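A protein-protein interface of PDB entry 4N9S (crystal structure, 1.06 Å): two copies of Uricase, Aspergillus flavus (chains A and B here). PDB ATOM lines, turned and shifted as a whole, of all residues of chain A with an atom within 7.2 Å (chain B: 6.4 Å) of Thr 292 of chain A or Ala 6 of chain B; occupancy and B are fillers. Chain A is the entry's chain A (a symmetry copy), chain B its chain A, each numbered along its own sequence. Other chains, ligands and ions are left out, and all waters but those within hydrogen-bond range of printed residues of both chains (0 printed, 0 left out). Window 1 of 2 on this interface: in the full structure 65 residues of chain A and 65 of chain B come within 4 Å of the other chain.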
ATOM      1  N   THR A 186      -1.986  26.343  32.285  1.00  0.00           N
ATOM      2  CA  THR A 186      -2.764  25.385  33.064  1.00  0.00           C
ATOM      3  C   THR A 186      -2.613  23.995  32.469  1.00  0.00           C
ATOM      4  O   THR A 186      -2.735  23.820  31.256  1.00  0.00           O
ATOM      5  CB  THR A 186      -4.255  25.760  33.034  1.00  0.00           C
ATOM      6  OG1 THR A 186      -4.429  27.059  33.592  1.00  0.00           O
ATOM      7  CG2 THR A 186      -5.096  24.776  33.808  1.00  0.00           C
ATOM      8  N   TYR A 233       2.117  27.116  21.307  1.00  0.00           N
ATOM      9  CA  TYR A 233       1.772  25.760  20.909  1.00  0.00           C
ATOM     10  C   TYR A 233       2.960  24.836  21.170  1.00  0.00           C
ATOM     11  O   TYR A 233       2.788  23.706  21.650  1.00  0.00           O
ATOM     12  CB  TYR A 233       1.338  25.716  19.440  1.00  0.00           C
ATOM     13  CG  TYR A 233       0.880  24.335  19.031  1.00  0.00           C
ATOM     14  CD1 TYR A 233      -0.397  23.891  19.348  1.00  0.00           C
ATOM     15  CD2 TYR A 233       1.734  23.469  18.376  1.00  0.00           C
ATOM     16  CE1 TYR A 233      -0.825  22.623  19.019  1.00  0.00           C
ATOM     17  CE2 TYR A 233       1.316  22.187  18.038  1.00  0.00           C
ATOM     18  CZ  TYR A 233       0.027  21.776  18.353  1.00  0.00           C
ATOM     19  OH  TYR A 233      -0.415  20.511  18.022  1.00  0.00           O
ATOM     20  N   ALA A 236       3.068  23.905  24.834  1.00  0.00           N
ATOM     21  CA  ALA A 236       2.032  22.954  25.210  1.00  0.00           C
ATOM     22  C   ALA A 236       2.363  21.548  24.735  1.00  0.00           C
ATOM     23  O   ALA A 236       2.183  20.580  25.477  1.00  0.00           O
ATOM     24  CB  ALA A 236       0.684  23.393  24.670  1.00  0.00           C
ATOM     25  N   LEU A 240       2.817  18.150  27.253  1.00  0.00           N
ATOM     26  CA  LEU A 240       2.043  16.923  27.061  1.00  0.00           C
ATOM     27  C   LEU A 240       2.952  15.713  26.831  1.00  0.00           C
ATOM     28  O   LEU A 240       2.674  14.618  27.312  1.00  0.00           O
ATOM     29  CB  LEU A 240       1.071  17.078  25.891  1.00  0.00           C
ATOM     30  CG  LEU A 240      -0.143  17.966  26.152  1.00  0.00           C
ATOM     31  CD1 LEU A 240      -0.888  18.258  24.859  1.00  0.00           C
ATOM     32  CD2 LEU A 240      -1.078  17.345  27.180  1.00  0.00           C
ATOM     33  N   GLU A 247      -4.073  15.635  30.487  1.00  0.00           N
ATOM     34  CA  GLU A 247      -4.884  15.501  29.282  1.00  0.00           C
ATOM     35  C   GLU A 247      -4.817  16.717  28.359  1.00  0.00           C
ATOM     36  O   GLU A 247      -4.858  16.561  27.142  1.00  0.00           O
ATOM     37  CB  GLU A 247      -6.330  15.224  29.665  1.00  0.00           C
ATOM     38  CG  GLU A 247      -6.470  13.873  30.378  1.00  0.00           C
ATOM     39  CD  GLU A 247      -7.895  13.512  30.762  1.00  0.00           C
ATOM     40  OE1 GLU A 247      -8.748  14.414  30.858  1.00  0.00           O
ATOM     41  OE2 GLU A 247      -8.151  12.310  30.979  1.00  0.00           O
ATOM     42  N   THR A 248      -4.758  17.918  28.922  1.00  0.00           N
ATOM     43  CA  THR A 248      -4.664  19.130  28.120  1.00  0.00           C
ATOM     44  C   THR A 248      -3.761  20.146  28.796  1.00  0.00           C
ATOM     45  O   THR A 248      -3.552  20.111  30.017  1.00  0.00           O
ATOM     46  CB  THR A 248      -6.034  19.798  27.882  1.00  0.00           C
ATOM     47  OG1 THR A 248      -6.602  20.218  29.120  1.00  0.00           O
ATOM     48  CG2 THR A 248      -7.004  18.877  27.174  1.00  0.00           C
ATOM     49  N   VAL A 249      -3.235  21.054  27.980  1.00  0.00           N
ATOM     50  CA  VAL A 249      -2.486  22.212  28.449  1.00  0.00           C
ATOM     51  C   VAL A 249      -3.100  23.442  27.796  1.00  0.00           C
ATOM     52  O   VAL A 249      -3.332  23.456  26.587  1.00  0.00           O
ATOM     53  CB  VAL A 249      -0.985  22.113  28.078  1.00  0.00           C
ATOM     54  CG1 VAL A 249      -0.245  23.391  28.448  1.00  0.00           C
ATOM     55  CG2 VAL A 249      -0.345  20.888  28.732  1.00  0.00           C
ATOM     56  N   GLU A 250      -3.360  24.463  28.607  1.00  0.00           N
ATOM     57  CA  GLU A 250      -3.948  25.696  28.136  1.00  0.00           C
ATOM     58  C   GLU A 250      -3.010  26.848  28.460  1.00  0.00           C
ATOM     59  O   GLU A 250      -2.495  26.941  29.572  1.00  0.00           O
ATOM     60  CB  GLU A 250      -5.295  25.886  28.827  1.00  0.00           C
ATOM     61  CG  GLU A 250      -6.026  27.145  28.467  1.00  0.00           C
ATOM     62  CD  GLU A 250      -7.157  27.443  29.442  1.00  0.00           C
ATOM     63  OE1 GLU A 250      -7.356  26.657  30.395  1.00  0.00           O
ATOM     64  OE2 GLU A 250      -7.837  28.473  29.268  1.00  0.00           O
ATOM     65  N   TYR A 251      -2.802  27.730  27.492  1.00  0.00           N
ATOM     66  CA  TYR A 251      -2.076  28.976  27.708  1.00  0.00           C
ATOM     67  C   TYR A 251      -2.998  30.149  27.434  1.00  0.00           C
ATOM     68  O   TYR A 251      -3.817  30.113  26.498  1.00  0.00           O
ATOM     69  CB  TYR A 251      -0.842  29.081  26.796  1.00  0.00           C
ATOM     70  CG  TYR A 251       0.387  28.385  27.316  1.00  0.00           C
ATOM     71  CD1 TYR A 251       1.345  29.079  28.054  1.00  0.00           C
ATOM     72  CD2 TYR A 251       0.593  27.041  27.091  1.00  0.00           C
ATOM     73  CE1 TYR A 251       2.473  28.452  28.540  1.00  0.00           C
ATOM     74  CE2 TYR A 251       1.704  26.409  27.579  1.00  0.00           C
ATOM     75  CZ  TYR A 251       2.640  27.109  28.307  1.00  0.00           C
ATOM     76  OH  TYR A 251       3.740  26.447  28.783  1.00  0.00           O
ATOM     77  N   LYS A 290      -4.946  32.767  23.148  1.00  0.00           N
ATOM     78  CA  LYS A 290      -5.299  31.613  23.964  1.00  0.00           C
ATOM     79  C   LYS A 290      -5.317  30.344  23.128  1.00  0.00           C
ATOM     80  O   LYS A 290      -5.693  30.355  21.939  1.00  0.00           O
ATOM     81  CB  LYS A 290      -6.697  31.788  24.565  1.00  0.00           C
ATOM     82  CG  LYS A 290      -6.822  32.978  25.493  1.00  0.00           C
ATOM     83  CD  LYS A 290      -8.253  33.119  26.002  1.00  0.00           C
ATOM     84  CE  LYS A 290      -8.454  34.307  26.907  1.00  0.00           C
ATOM     85  NZ  LYS A 290      -8.121  33.997  28.320  1.00  0.00           N
ATOM     86  N   CYS A 291      -4.940  29.229  23.742  1.00  0.00           N
ATOM     87  CA  CYS A 291      -5.235  27.948  23.149  1.00  0.00           C
ATOM     88  C   CYS A 291      -5.186  26.848  24.183  1.00  0.00           C
ATOM     89  O   CYS A 291      -4.552  26.944  25.236  1.00  0.00           O
ATOM     90  CB  CYS A 291      -4.284  27.629  22.010  1.00  0.00           C
ATOM     91  SG  CYS A 291      -2.643  27.304  22.586  1.00  0.00           S
ATOM     92  N   THR A 292      -5.958  25.820  23.872  1.00  0.00           N
ATOM     93  CA  THR A 292      -6.014  24.581  24.633  1.00  0.00           C
ATOM     94  C   THR A 292      -5.557  23.469  23.708  1.00  0.00           C
ATOM     95  O   THR A 292      -6.113  23.287  22.624  1.00  0.00           O
ATOM     96  CB  THR A 292      -7.422  24.265  25.132  1.00  0.00           C
ATOM     97  OG1 THR A 292      -7.859  25.360  25.935  1.00  0.00           O
ATOM     98  CG2 THR A 292      -7.434  22.979  25.970  1.00  0.00           C
ATOM     99  N   VAL A 293      -4.528  22.750  24.134  1.00  0.00           N
ATOM    100  CA  VAL A 293      -3.906  21.704  23.341  1.00  0.00           C
ATOM    101  C   VAL A 293      -4.128  20.373  24.044  1.00  0.00           C
ATOM    102  O   VAL A 293      -3.977  20.263  25.261  1.00  0.00           O
ATOM    103  CB  VAL A 293      -2.398  21.986  23.167  1.00  0.00           C
ATOM    104  CG1 VAL A 293      -1.736  20.927  22.313  1.00  0.00           C
ATOM    105  CG2 VAL A 293      -2.175  23.370  22.547  1.00  0.00           C
ATOM    106  N   GLY A 294      -4.521  19.372  23.268  1.00  0.00           N
ATOM    107  CA  GLY A 294      -4.727  18.040  23.771  1.00  0.00           C
ATOM    108  C   GLY A 294      -3.991  17.060  22.905  1.00  0.00           C
ATOM    109  O   GLY A 294      -3.223  17.439  22.028  1.00  0.00           O
ATOM    110  N   ALA B   3      -2.756  18.283  19.259  1.00  0.00           N
ATOM    111  CA  ALA B   3      -3.640  19.032  18.377  1.00  0.00           C
ATOM    112  C   ALA B   3      -4.325  20.155  19.152  1.00  0.00           C
ATOM    113  O   ALA B   3      -4.509  20.089  20.386  1.00  0.00           O
ATOM    114  CB  ALA B   3      -4.689  18.119  17.750  1.00  0.00           C
ATOM    115  N   VAL B   4      -4.691  21.203  18.430  1.00  0.00           N
ATOM    116  CA  VAL B   4      -5.467  22.279  19.018  1.00  0.00           C
ATOM    117  C   VAL B   4      -6.894  21.807  19.299  1.00  0.00           C
ATOM    118  O   VAL B   4      -7.599  21.362  18.394  1.00  0.00           O
ATOM    119  CB  VAL B   4      -5.500  23.486  18.085  1.00  0.00           C
ATOM    120  CG1 VAL B   4      -6.427  24.568  18.624  1.00  0.00           C
ATOM    121  CG2 VAL B   4      -4.080  24.027  17.860  1.00  0.00           C
ATOM    122  N   LYS B   5      -7.303  21.870  20.560  1.00  0.00           N
ATOM    123  CA  LYS B   5      -8.669  21.530  20.932  1.00  0.00           C
ATOM    124  C   LYS B   5      -9.572  22.769  20.964  1.00  0.00           C
ATOM    125  O   LYS B   5     -10.771  22.666  20.663  1.00  0.00           O
ATOM    126  CB  LYS B   5      -8.695  20.814  22.281  1.00  0.00           C
ATOM    127  CG  LYS B   5      -7.885  19.518  22.310  1.00  0.00           C
ATOM    128  CD  LYS B   5      -8.421  18.467  21.338  1.00  0.00           C
ATOM    129  CE  LYS B   5      -7.634  17.160  21.444  1.00  0.00           C
ATOM    130  NZ  LYS B   5      -6.214  17.320  21.048  1.00  0.00           N
ATOM    131  N   ALA B   6      -9.005  23.926  21.313  1.00  0.00           N
ATOM    132  CA  ALA B   6      -9.743  25.179  21.337  1.00  0.00           C
ATOM    133  C   ALA B   6      -8.736  26.289  21.140  1.00  0.00           C
ATOM    134  O   ALA B   6      -7.592  26.168  21.573  1.00  0.00           O
ATOM    135  CB  ALA B   6     -10.449  25.371  22.658  1.00  0.00           C
ATOM    136  N   ALA B   7      -9.157  27.378  20.511  1.00  0.00           N
ATOM    137  CA  ALA B   7      -8.295  28.534  20.357  1.00  0.00           C
ATOM    138  C   ALA B   7      -9.137  29.774  20.127  1.00  0.00           C
ATOM    139  O   ALA B   7     -10.137  29.735  19.399  1.00  0.00           O
ATOM    140  CB  ALA B   7      -7.339  28.327  19.201  1.00  0.00           C
ATOM    141  N   ARG B   8      -8.703  30.892  20.716  1.00  0.00           N
ATOM    142  CA  ARG B   8      -9.272  32.187  20.396  1.00  0.00           C
ATOM    143  C   ARG B   8      -8.214  33.235  20.655  1.00  0.00           C
ATOM    144  O   ARG B   8      -7.305  33.026  21.459  1.00  0.00           O
ATOM    145  CB  ARG B   8     -10.554  32.487  21.170  1.00  0.00           C
ATOM    146  CG  ARG B   8     -10.404  32.621  22.670  1.00  0.00           C
ATOM    147  CD  ARG B   8     -11.743  32.871  23.357  1.00  0.00           C
ATOM    148  NE  ARG B   8     -12.599  31.695  23.255  1.00  0.00           N
ATOM    149  CZ  ARG B   8     -13.855  31.620  23.688  1.00  0.00           C
ATOM    150  NH1 ARG B   8     -14.441  32.660  24.256  1.00  0.00           N
ATOM    151  NH2 ARG B   8     -14.541  30.490  23.546  1.00  0.00           N
ATOM    152  N   GLU B  40     -12.646  33.235  16.983  1.00  0.00           N
ATOM    153  CA  GLU B  40     -12.421  31.814  16.748  1.00  0.00           C
ATOM    154  C   GLU B  40     -12.729  31.480  15.301  1.00  0.00           C
ATOM    155  O   GLU B  40     -13.542  32.148  14.660  1.00  0.00           O
ATOM    156  CB  GLU B  40     -13.372  30.944  17.560  1.00  0.00           C
ATOM    157  CG  GLU B  40     -13.213  30.942  19.047  1.00  0.00           C
ATOM    158  CD  GLU B  40     -14.158  29.908  19.617  1.00  0.00           C
ATOM    159  OE1 GLU B  40     -13.838  28.697  19.592  1.00  0.00           O
ATOM    160  OE2 GLU B  40     -15.268  30.289  20.008  1.00  0.00           O
ATOM    161  N   TYR B  47      -1.199  28.356  14.987  1.00  0.00           N
ATOM    162  CA  TYR B  47      -0.571  27.725  16.142  1.00  0.00           C
ATOM    163  C   TYR B  47       0.347  26.576  15.722  1.00  0.00           C
ATOM    164  O   TYR B  47       1.455  26.439  16.251  1.00  0.00           O
ATOM    165  CB  TYR B  47      -1.635  27.205  17.116  1.00  0.00           C
ATOM    166  CG  TYR B  47      -2.530  28.281  17.704  1.00  0.00           C
ATOM    167  CD1 TYR B  47      -3.632  28.747  17.013  1.00  0.00           C
ATOM    168  CD2 TYR B  47      -2.279  28.820  18.967  1.00  0.00           C
ATOM    169  CE1 TYR B  47      -4.458  29.733  17.552  1.00  0.00           C
ATOM    170  CE2 TYR B  47      -3.105  29.786  19.503  1.00  0.00           C
ATOM    171  CZ  TYR B  47      -4.195  30.235  18.805  1.00  0.00           C
ATOM    172  OH  TYR B  47      -5.033  31.185  19.322  1.00  0.00           O
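The backbone carbonyl oxygen of Ala 3 of chain B sits at hydrogen-bond distance from the side-chain amino group of Lys 5 of chain B. NH2 of Arg 8 of chain B is in salt-bridge range of OE2 of Glu 40 of chain B, 3.6 Å away. The backbone carbonyl oxygen (O) of Val 249 of chain A lies within hydrogen-bond range of the backbone NH (N) of Val 293 of chain A (2.8 Å). The backbone NH (N) of Tyr 251 of chain A is in hydrogen-bond range of the backbone carbonyl oxygen (O) of Cys 291 of chain A.
Leu 240 of chain A touches none of the printed residues of chain B. Printed residues of chain B within 4 Å of Lys 290 of chain A: Ala 7 (3.5 Å), Arg 8 (2.9 Å) and Tyr 47 (2.8 Å). Of the printed residues of chain B, Thr 292 of chain A touches Val 4 (3.7 Å), Lys 5 (2.8 Å) and Ala 6 (2.8 Å). Of the printed residues of chain B, Val 293 of chain A touches Ala 3. Printed residues of chain A within 4 Å of Ala 6 of chain B: Cys 291 and Thr 292. Glu 40 of chain B touches none of the printed residues of chain A. The nearest printed residue of chain B that does not touch Thr 292 of chain A is Ala 3 of chain B (4.2 Å).
Tyr 233 of chain A touches Val 4 of chain B. O of Tyr 47 of chain B touches CB of Tyr 233 of chain A, at 3.3 Å. Lys 290 of chain A touches Ala 7 of chain B. Cys 291 of chain A touches Ala 6 of chain B. Cys 291 of chain A touches Tyr 47 of chain B (CB to CE2, 3.5 Å). C of Val 4 of chain B touches O of Thr 292 of chain A, 3.7 Å away. Val 293 of chain A touches Ala 3 of chain B (CA to O, 3.4 Å).
No position is printed for both chains. Of the 14 pairs that touch across the chains among the printed residues, none has its exchanged pair printed and touching as well.
The backbone NH (N) of Ala 3 of chain B sits at hydrogen-bond distance from the side-chain hydroxyl (OH) of Tyr 233 of chain A (3.5 Å). The backbone NH of Ala 3 of chain B lies within hydrogen-bond range of the backbone carbonyl oxygen of Gly 294 of chain A. The backbone NH (N) of Lys 5 of chain B sits at hydrogen-bond distance from the backbone carbonyl oxygen (O) of Thr 292 of chain A, at 2.8 Å. The backbone carbonyl oxygen (O) of Gly 294 of chain A sits close to the side-chain amino group (NZ) of Lys 5 of chain B (3.1 Å). O of Ala 6 of chain B lies within hydrogen-bond range of N of Thr 292 of chain A (2.8 Å). N of Lys 290 of chain A is in hydrogen-bond range of O of Arg 8 of chain B (2.9 Å). O of Lys 290 of chain A lies within hydrogen-bond range of OH of Tyr 47 of chain B, 2.8 Å away.
Hydrophobic or aromatic side chains of chain A that line the printed part of chain B: Tyr 233 and Val 293. Along chain A the printed residues that touch a printed residue of chain B span positions 233 to 294. Printed residues of chain B that touch a printed residue of chain A: Ala 3, Val 4, Lys 5, Ala 6, Ala 7, Arg 8 and Tyr 47. Hydrophobic or aromatic side chains of chain B within 4 Å of the printed part of chain A: Val 4, Ala 7 and Tyr 47.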
